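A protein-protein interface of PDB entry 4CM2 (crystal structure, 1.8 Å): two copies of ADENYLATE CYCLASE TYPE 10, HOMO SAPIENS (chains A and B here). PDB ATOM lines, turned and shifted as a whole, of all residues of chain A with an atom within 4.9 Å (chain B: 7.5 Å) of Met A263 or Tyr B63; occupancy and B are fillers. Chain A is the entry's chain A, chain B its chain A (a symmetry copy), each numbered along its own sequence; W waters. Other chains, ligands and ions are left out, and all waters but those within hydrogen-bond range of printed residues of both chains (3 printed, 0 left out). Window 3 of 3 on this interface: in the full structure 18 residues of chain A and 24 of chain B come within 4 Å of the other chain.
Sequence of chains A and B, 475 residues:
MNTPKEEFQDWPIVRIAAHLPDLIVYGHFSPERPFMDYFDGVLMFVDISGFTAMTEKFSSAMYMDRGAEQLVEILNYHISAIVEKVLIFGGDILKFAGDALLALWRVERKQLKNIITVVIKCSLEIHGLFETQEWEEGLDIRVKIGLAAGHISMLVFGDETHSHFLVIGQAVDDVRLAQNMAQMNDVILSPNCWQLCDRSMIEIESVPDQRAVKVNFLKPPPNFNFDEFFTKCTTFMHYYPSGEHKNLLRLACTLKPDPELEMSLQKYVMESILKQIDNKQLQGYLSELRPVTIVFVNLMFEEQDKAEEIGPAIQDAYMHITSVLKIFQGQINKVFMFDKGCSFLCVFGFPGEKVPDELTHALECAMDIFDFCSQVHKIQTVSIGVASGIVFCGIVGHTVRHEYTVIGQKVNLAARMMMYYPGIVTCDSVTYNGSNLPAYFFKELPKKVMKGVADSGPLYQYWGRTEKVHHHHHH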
ATOM      1  N   PRO A 259      22.469   7.667   5.861  1.00  0.00           N
ATOM      2  CA  PRO A 259      23.676   8.494   5.649  1.00  0.00           C
ATOM      3  C   PRO A 259      24.272   8.368   4.285  1.00  0.00           C
ATOM      4  O   PRO A 259      24.782   9.325   3.783  1.00  0.00           O
ATOM      5  CB  PRO A 259      24.665   7.964   6.712  1.00  0.00           C
ATOM      6  CG  PRO A 259      23.816   7.268   7.730  1.00  0.00           C
ATOM      7  CD  PRO A 259      22.530   6.848   7.104  1.00  0.00           C
ATOM      8  N   GLU A 260      24.191   7.174   3.673  1.00  0.00           N
ATOM      9  CA  GLU A 260      24.769   7.020   2.337  1.00  0.00           C
ATOM     10  C   GLU A 260      23.942   7.802   1.278  1.00  0.00           C
ATOM     11  O   GLU A 260      24.523   8.462   0.395  1.00  0.00           O
ATOM     12  CB  GLU A 260      24.909   5.541   1.927  1.00  0.00           C
ATOM     13  CG  GLU A 260      26.058   4.833   2.631  1.00  0.00           C
ATOM     14  CD  GLU A 260      27.386   5.213   2.063  1.00  0.00           C
ATOM     15  OE1 GLU A 260      27.428   5.539   0.871  1.00  0.00           O
ATOM     16  OE2 GLU A 260      28.400   5.141   2.788  1.00  0.00           O
ATOM     17  N   LEU A 261      22.650   7.856   1.442  1.00  0.00           N
ATOM     18  CA  LEU A 261      21.769   8.604   0.540  1.00  0.00           C
ATOM     19  C   LEU A 261      22.013  10.091   0.781  1.00  0.00           C
ATOM     20  O   LEU A 261      22.176  10.860  -0.132  1.00  0.00           O
ATOM     21  CB  LEU A 261      20.348   8.281   0.750  1.00  0.00           C
ATOM     22  CG  LEU A 261      19.398   9.001  -0.202  1.00  0.00           C
ATOM     23  CD1 LEU A 261      19.688   8.919  -1.701  1.00  0.00           C
ATOM     24  CD2 LEU A 261      17.935   8.635   0.127  1.00  0.00           C
ATOM     25  N   GLU A 262      22.053  10.501   2.032  1.00  0.00           N
ATOM     26  CA  GLU A 262      22.280  11.941   2.311  1.00  0.00           C
ATOM     27  C   GLU A 262      23.624  12.405   1.828  1.00  0.00           C
ATOM     28  O   GLU A 262      23.724  13.544   1.300  1.00  0.00           O
ATOM     29  CB  GLU A 262      22.172  12.215   3.794  1.00  0.00           C
ATOM     30  CG  GLU A 262      22.313  13.674   4.207  1.00  0.00           C
ATOM     31  CD  GLU A 262      21.852  14.020   5.618  1.00  0.00           C
ATOM     32  OE1 GLU A 262      20.839  13.371   6.074  1.00  0.00           O
ATOM     33  OE2 GLU A 262      22.491  14.937   6.235  1.00  0.00           O
ATOM     34  N   MET A 263      24.667  11.612   2.004  1.00  0.00           N
ATOM     35  CA  MET A 263      25.954  11.994   1.417  1.00  0.00           C
ATOM     36  C   MET A 263      25.878  12.261  -0.079  1.00  0.00           C
ATOM     37  O   MET A 263      26.527  13.187  -0.589  1.00  0.00           O
ATOM     38  CB  MET A 263      27.077  10.964   1.706  1.00  0.00           C
ATOM     39  CG  MET A 263      27.835  11.150   2.993  1.00  0.00           C
ATOM     40  SD  MET A 263      29.215   9.962   3.055  1.00  0.00           S
ATOM     41  CE  MET A 263      29.695   9.957   1.346  1.00  0.00           C
ATOM     42  N   SER A 264      25.169  11.428  -0.799  1.00  0.00           N
ATOM     43  CA  SER A 264      24.984  11.627  -2.227  1.00  0.00           C
ATOM     44  C   SER A 264      24.117  12.861  -2.563  1.00  0.00           C
ATOM     45  O   SER A 264      24.487  13.729  -3.401  1.00  0.00           O
ATOM     46  CB  SER A 264      24.449  10.328  -2.840  1.00  0.00           C
ATOM     47  OG  SER A 264      23.861  10.629  -4.074  1.00  0.00           O
ATOM     48  N   LEU A 265      23.004  13.051  -1.848  1.00  0.00           N
ATOM     49  CA  LEU A 265      22.159  14.193  -2.159  1.00  0.00           C
ATOM     50  C   LEU A 265      22.688  15.555  -1.731  1.00  0.00           C
ATOM     51  O   LEU A 265      22.491  16.585  -2.431  1.00  0.00           O
ATOM     52  CB  LEU A 265      20.760  13.988  -1.448  1.00  0.00           C
ATOM     53  CG  LEU A 265      19.967  12.761  -1.894  1.00  0.00           C
ATOM     54  CD1 LEU A 265      18.626  12.738  -1.129  1.00  0.00           C
ATOM     55  CD2 LEU A 265      19.762  12.638  -3.372  1.00  0.00           C
ATOM     56  N   GLN A 266      23.521  15.631  -0.681  1.00  0.00           N
ATOM     57  CA  GLN A 266      23.957  16.951  -0.254  1.00  0.00           C
ATOM     58  C   GLN A 266      24.910  17.552  -1.290  1.00  0.00           C
ATOM     59  O   GLN A 266      25.089  18.750  -1.255  1.00  0.00           O
ATOM     60  CB  GLN A 266      24.608  16.894   1.077  1.00  0.00           C
ATOM     61  CG  GLN A 266      25.975  16.245   1.097  1.00  0.00           C
ATOM     62  CD  GLN A 266      26.826  16.679   2.261  1.00  0.00           C
ATOM     63  OE1 GLN A 266      26.573  16.290   3.382  1.00  0.00           O
ATOM     64  NE2 GLN A 266      27.799  17.577   1.997  1.00  0.00           N
ATOM     65  N   LYS A 267      25.486  16.721  -2.151  1.00  0.00           N
ATOM     66  CA  LYS A 267      26.496  17.199  -3.149  1.00  0.00           C
ATOM     67  C   LYS A 267      25.868  18.129  -4.163  1.00  0.00           C
ATOM     68  O   LYS A 267      26.566  18.954  -4.799  1.00  0.00           O
ATOM     69  CB  LYS A 267      27.153  16.035  -3.822  1.00  0.00           C
ATOM     70  CG  LYS A 267      27.958  15.187  -2.861  1.00  0.00           C
ATOM     71  CD  LYS A 267      28.715  14.095  -3.574  1.00  0.00           C
ATOM     72  CE  LYS A 267      29.400  13.132  -2.546  1.00  0.00           C
ATOM     73  NZ  LYS A 267      30.233  12.175  -3.311  1.00  0.00           N
ATOM     74  N   MET B  54      29.400   4.215  16.045  1.00  0.00           N
ATOM     75  CA  MET B  54      29.416   4.920  14.740  1.00  0.00           C
ATOM     76  C   MET B  54      30.152   6.311  14.728  1.00  0.00           C
ATOM     77  O   MET B  54      30.413   6.858  13.655  1.00  0.00           O
ATOM     78  CB  MET B  54      27.977   5.105  14.219  1.00  0.00           C
ATOM     79  CG  MET B  54      27.350   3.921  13.480  1.00  0.00           C
ATOM     80  SD  MET B  54      25.693   4.482  12.902  1.00  0.00           S
ATOM     81  CE  MET B  54      24.740   4.885  14.365  1.00  0.00           C
ATOM     82  N   GLU B  56      33.153   6.853  14.971  1.00  0.00           N
ATOM     83  CA  GLU B  56      34.335   6.685  14.117  1.00  0.00           C
ATOM     84  C   GLU B  56      34.075   6.818  12.607  1.00  0.00           C
ATOM     85  O   GLU B  56      34.758   7.566  11.933  1.00  0.00           O
ATOM     86  CB  GLU B  56      34.999   5.326  14.402  1.00  0.00           C
ATOM     87  CG  GLU B  56      35.806   5.341  15.699  1.00  0.00           C
ATOM     88  CD  GLU B  56      36.786   6.496  15.741  1.00  0.00           C
ATOM     89  OE1 GLU B  56      37.443   6.762  14.712  1.00  0.00           O
ATOM     90  OE2 GLU B  56      36.911   7.136  16.800  1.00  0.00           O
ATOM     91  N   LYS B  57      33.150   6.028  12.118  1.00  0.00           N
ATOM     92  CA  LYS B  57      32.588   6.121  10.747  1.00  0.00           C
ATOM     93  C   LYS B  57      32.360   7.612  10.332  1.00  0.00           C
ATOM     94  O   LYS B  57      32.773   8.054   9.249  1.00  0.00           O
ATOM     95  CB  LYS B  57      31.267   5.359  10.753  1.00  0.00           C
ATOM     96  CG  LYS B  57      30.513   5.305   9.439  1.00  0.00           C
ATOM     97  CD  LYS B  57      29.119   4.687   9.627  1.00  0.00           C
ATOM     98  CE  LYS B  57      28.350   4.710   8.317  1.00  0.00           C
ATOM     99  NZ  LYS B  57      27.931   3.354   7.880  1.00  0.00           N
ATOM    100  N   PHE B  58      31.742   8.391  11.230  1.00  0.00           N
ATOM    101  CA  PHE B  58      31.312   9.791  10.889  1.00  0.00           C
ATOM    102  C   PHE B  58      32.380  10.829  10.989  1.00  0.00           C
ATOM    103  O   PHE B  58      32.251  11.980  10.558  1.00  0.00           O
ATOM    104  CB  PHE B  58      30.007  10.122  11.671  1.00  0.00           C
ATOM    105  CG  PHE B  58      28.789   9.475  11.133  1.00  0.00           C
ATOM    106  CD1 PHE B  58      28.201   9.901   9.998  1.00  0.00           C
ATOM    107  CD2 PHE B  58      28.219   8.395  11.770  1.00  0.00           C
ATOM    108  CE1 PHE B  58      27.084   9.277   9.468  1.00  0.00           C
ATOM    109  CE2 PHE B  58      27.101   7.808  11.292  1.00  0.00           C
ATOM    110  CZ  PHE B  58      26.525   8.207  10.116  1.00  0.00           C
ATOM    111  N   SER B  59      33.570  10.473  11.509  1.00  0.00           N
ATOM    112  CA  SER B  59      34.697  11.395  11.357  1.00  0.00           C
ATOM    113  C   SER B  59      35.446  11.215   9.999  1.00  0.00           C
ATOM    114  O   SER B  59      36.199  12.057   9.615  1.00  0.00           O
ATOM    115  CB  SER B  59      35.715  11.271  12.531  1.00  0.00           C
ATOM    116  OG  SER B  59      35.592  12.428  13.417  1.00  0.00           O
ATOM    117  N   SER B  60      35.116  10.184   9.234  1.00  0.00           N
ATOM    118  CA  SER B  60      35.660  10.088   7.855  1.00  0.00           C
ATOM    119  C   SER B  60      35.469  11.415   7.026  1.00  0.00           C
ATOM    120  O   SER B  60      34.387  12.059   7.033  1.00  0.00           O
ATOM    121  CB  SER B  60      34.943   8.983   7.151  1.00  0.00           C
ATOM    122  OG  SER B  60      35.342   8.984   5.811  1.00  0.00           O
ATOM    123  N   ALA B  61      36.460  11.783   6.227  1.00  0.00           N
ATOM    124  CA  ALA B  61      36.323  12.812   5.200  1.00  0.00           C
ATOM    125  C   ALA B  61      35.169  12.587   4.226  1.00  0.00           C
ATOM    126  O   ALA B  61      34.716  13.516   3.508  1.00  0.00           O
ATOM    127  CB  ALA B  61      37.629  12.919   4.389  1.00  0.00           C
ATOM    128  N   MET B  62      34.683  11.351   4.141  1.00  0.00           N
ATOM    129  CA  MET B  62      33.561  11.034   3.250  1.00  0.00           C
ATOM    130  C   MET B  62      32.328  11.882   3.606  1.00  0.00           C
ATOM    131  O   MET B  62      31.479  12.148   2.733  1.00  0.00           O
ATOM    132  CB  MET B  62      33.217   9.533   3.313  1.00  0.00           C
ATOM    133  CG  MET B  62      34.208   8.599   2.567  1.00  0.00           C
ATOM    134  SD  MET B  62      34.293   8.900   0.802  1.00  0.00           S
ATOM    135  CE  MET B  62      32.778   8.137   0.205  1.00  0.00           C
ATOM    136  N   TYR B  63      32.255  12.280   4.877  1.00  0.00           N
ATOM    137  CA  TYR B  63      31.045  13.013   5.403  1.00  0.00           C
ATOM    138  C   TYR B  63      31.201  14.559   5.234  1.00  0.00           C
ATOM    139  O   TYR B  63      30.256  15.312   5.549  1.00  0.00           O
ATOM    140  CB  TYR B  63      30.706  12.680   6.836  1.00  0.00           C
ATOM    141  CG  TYR B  63      30.128  11.296   6.880  1.00  0.00           C
ATOM    142  CD1 TYR B  63      28.825  11.061   6.496  1.00  0.00           C
ATOM    143  CD2 TYR B  63      30.966  10.196   7.181  1.00  0.00           C
ATOM    144  CE1 TYR B  63      28.344   9.780   6.383  1.00  0.00           C
ATOM    145  CE2 TYR B  63      30.465   8.904   7.176  1.00  0.00           C
ATOM    146  CZ  TYR B  63      29.174   8.688   6.750  1.00  0.00           C
ATOM    147  OH  TYR B  63      28.628   7.418   6.707  1.00  0.00           O
ATOM    148  N   MET B  64      32.251  14.940   4.551  1.00  0.00           N
ATOM    149  CA  MET B  64      32.405  16.323   4.044  1.00  0.00           C
ATOM    150  C   MET B  64      32.054  17.370   5.131  1.00  0.00           C
ATOM    151  O   MET B  64      31.335  18.328   4.868  1.00  0.00           O
ATOM    152  CB  MET B  64      31.489  16.560   2.894  1.00  0.00           C
ATOM    153  CG  MET B  64      31.893  15.820   1.628  1.00  0.00           C
ATOM    154  SD  MET B  64      30.696  15.620   0.349  1.00  0.00           S
ATOM    155  CE  MET B  64      29.454  14.578   1.097  1.00  0.00           C
ATOM    156  N   ASP B  65      32.634  17.269   6.269  1.00  0.00           N
ATOM    157  CA  ASP B  65      32.300  18.318   7.252  1.00  0.00           C
ATOM    158  C   ASP B  65      30.866  18.378   7.805  1.00  0.00           C
ATOM    159  O   ASP B  65      30.601  19.236   8.642  1.00  0.00           O
ATOM    160  CB  ASP B  65      32.770  19.694   6.818  1.00  0.00           C
ATOM    161  CG  ASP B  65      34.279  19.679   6.474  1.00  0.00           C
ATOM    162  OD1 ASP B  65      35.081  19.006   7.182  1.00  0.00           O
ATOM    163  OD2 ASP B  65      34.625  20.305   5.492  1.00  0.00           O
ATOM    164  N   ARG B  66      30.014  17.391   7.481  1.00  0.00           N
ATOM    165  CA  ARG B  66      28.732  17.262   8.163  1.00  0.00           C
ATOM    166  C   ARG B  66      28.656  15.938   8.889  1.00  0.00           C
ATOM    167  O   ARG B  66      27.592  15.510   9.184  1.00  0.00           O
ATOM    168  CB  ARG B  66      27.556  17.381   7.165  1.00  0.00           C
ATOM    169  CG  ARG B  66      27.443  18.796   6.536  1.00  0.00           C
ATOM    170  CD  ARG B  66      26.257  18.954   5.588  1.00  0.00           C
ATOM    171  NE  ARG B  66      25.021  18.731   6.289  1.00  0.00           N
ATOM    172  CZ  ARG B  66      24.253  17.645   6.253  1.00  0.00           C
ATOM    173  NH1 ARG B  66      24.501  16.635   5.430  1.00  0.00           N
ATOM    174  NH2 ARG B  66      23.177  17.574   7.010  1.00  0.00           N
ATOM    175  N   GLY B  67      29.796  15.413   9.386  1.00  0.00           N
ATOM    176  CA  GLY B  67      29.662  14.230  10.230  1.00  0.00           C
ATOM    177  C   GLY B  67      28.845  14.357  11.442  1.00  0.00           C
ATOM    178  O   GLY B  67      28.151  13.439  11.774  1.00  0.00           O
ATOM    179  N   ALA B  68      28.974  15.458  12.190  1.00  0.00           N
ATOM    180  CA  ALA B  68      28.213  15.556  13.386  1.00  0.00           C
ATOM    181  C   ALA B  68      26.727  15.628  13.151  1.00  0.00           C
ATOM    182  O   ALA B  68      25.931  15.020  13.908  1.00  0.00           O
ATOM    183  CB  ALA B  68      28.625  16.773  14.201  1.00  0.00           C
ATOM    184  N   GLU B  69      26.384  16.369  12.140  1.00  0.00           N
ATOM    185  CA  GLU B  69      24.964  16.505  11.752  1.00  0.00           C
ATOM    186  C   GLU B  69      24.346  15.175  11.279  1.00  0.00           C
ATOM    187  O   GLU B  69      23.256  14.768  11.695  1.00  0.00           O
ATOM    188  CB  GLU B  69      24.891  17.530  10.683  1.00  0.00           C
ATOM    189  CG  GLU B  69      25.271  18.970  11.172  1.00  0.00           C
ATOM    190  CD  GLU B  69      26.701  19.324  11.183  1.00  0.00           C
ATOM    191  OE1 GLU B  69      27.618  18.513  10.854  1.00  0.00           O
ATOM    192  OE2 GLU B  69      27.056  20.503  11.542  1.00  0.00           O
ATOM    193  N   GLN B  70      25.106  14.446  10.473  1.00  0.00           N
ATOM    194  CA  GLN B  70      24.651  13.129  10.026  1.00  0.00           C
ATOM    195  C   GLN B  70      24.559  12.147  11.184  1.00  0.00           C
ATOM    196  O   GLN B  70      23.604  11.321  11.319  1.00  0.00           O
ATOM    197  CB  GLN B  70      25.601  12.607   8.975  1.00  0.00           C
ATOM    198  CG  GLN B  70      25.412  13.281   7.625  1.00  0.00           C
ATOM    199  CD  GLN B  70      24.954  12.331   6.563  1.00  0.00           C
ATOM    200  OE1 GLN B  70      24.013  11.538   6.729  1.00  0.00           O
ATOM    201  NE2 GLN B  70      25.582  12.454   5.436  1.00  0.00           N
ATOM    202  N   LEU B  71      25.586  12.216  12.082  1.00  0.00           N
ATOM    203  CA  LEU B  71      25.541  11.325  13.240  1.00  0.00           C
ATOM    204  C   LEU B  71      24.355  11.514  14.132  1.00  0.00           C
ATOM    205  O   LEU B  71      23.685  10.493  14.481  1.00  0.00           O
ATOM    206  CB  LEU B  71      26.846  11.406  14.059  1.00  0.00           C
ATOM    207  CG  LEU B  71      26.921  10.442  15.263  1.00  0.00           C
ATOM    208  CD1 LEU B  71      26.814   8.978  14.871  1.00  0.00           C
ATOM    209  CD2 LEU B  71      28.282  10.638  15.862  1.00  0.00           C
ATOM    210  N   LEU B 289      31.326  17.977  16.222  1.00  0.00           N
ATOM    211  CA  LEU B 289      32.537  17.187  16.507  1.00  0.00           C
ATOM    212  C   LEU B 289      33.544  18.168  16.989  1.00  0.00           C
ATOM    213  O   LEU B 289      33.938  19.083  16.228  1.00  0.00           O
ATOM    214  CB  LEU B 289      33.073  16.542  15.226  1.00  0.00           C
ATOM    215  CG  LEU B 289      32.188  15.480  14.731  1.00  0.00           C
ATOM    216  CD1 LEU B 289      32.601  14.857  13.397  1.00  0.00           C
ATOM    217  CD2 LEU B 289      32.117  14.441  15.758  1.00  0.00           C
HETATM  218  O   HOH W   1      27.738  14.205   4.726  1.00  0.00           O
HETATM  219  O   HOH W   2      28.848  18.549  -0.553  1.00  0.00           O
HETATM  220  O   HOH W   3      29.470  19.583   3.489  1.00  0.00           O
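Among the printed residues, merely in contact across the chains: Pro A259 with Phe B58, Pro A259 with Gln B70, Glu A262 with Gln B70, Met A263 with Tyr B63, Met A263 with Met B64, Met A263 with Gln B70, Gln A266 with Met B64 and Lys A267 with Met B64.
The backbone NH (N) of Met B62 lies within hydrogen-bond range of the side-chain hydroxyl (OG) of Ser B60, at 3.0 Å.
Of the 9 printed residues of chain A, 5 touch a printed residue of chain B. Of the 18 printed residues of chain B, 6 touch a printed residue of chain A. Among the printed residues, 11 pairs touch across the chains. Among the printed residues, Asp or Glu carboxylates within 4 Å of a Lys or Arg side-chain nitrogen of the other chain: Glu A262 with Arg B66.
Water W3 lies within hydrogen-bond range of O of Met B64 (2.6 Å) and NE2 of Gln A266 (3.0 Å). Water W1 lies within hydrogen-bond range of the side-chain amide oxygen (OE1) of Gln A266 (2.7 Å), the side-chain amide nitrogen (NE2) of Gln B70 (2.9 Å) and the backbone carbonyl oxygen (O) of Tyr B63 (2.9 Å). Water W2 bridges the side-chain amide nitrogen (NE2) of Gln A266 and the side-chain sulfur (SD) of Met B64.
Printed residues of chain B within 4 Å of Pro A259: Phe B58 and Gln B70. Of the printed residues of chain B, Glu A262 touches Arg B66 and Gln B70. Of the printed residues of chain B, Met A263 touches Met B62, Tyr B63, Met B64 and Gln B70. Ser A264 touches none of the printed residues of chain B. Leu A265 touches none of the printed residues of chain B. Of the printed residues of chain A, Met B62 touches Met A263 (3.1 Å). Of the printed residues of chain A, Gln B70 touches Pro A259 (3.2 Å), Glu A262 (3.5 Å) and Met A263 (3.6 Å). The nearest printed residue of chain A that does not touch Tyr B63 is Pro A259 (4.0004 Å). The nearest printed residue of chain B that does not touch Lys A267 is Met B62 (5.8 Å).
The side-chain carboxylate (OE2) of Glu A262 lies within salt-bridge range of the guanidinium group (NH1) of Arg B66, 2.8 Å away. The side-chain amide oxygen of Gln A266 sits at hydrogen-bond distance from the guanidinium group of Arg B66, 2.9 Å away. SD of Met A263 sits close to O of Met B62, at 3.2 Å.
No position is printed for both chains. Of the 11 pairs that touch across the chains among the printed residues, none has its exchanged pair printed and touching as well.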
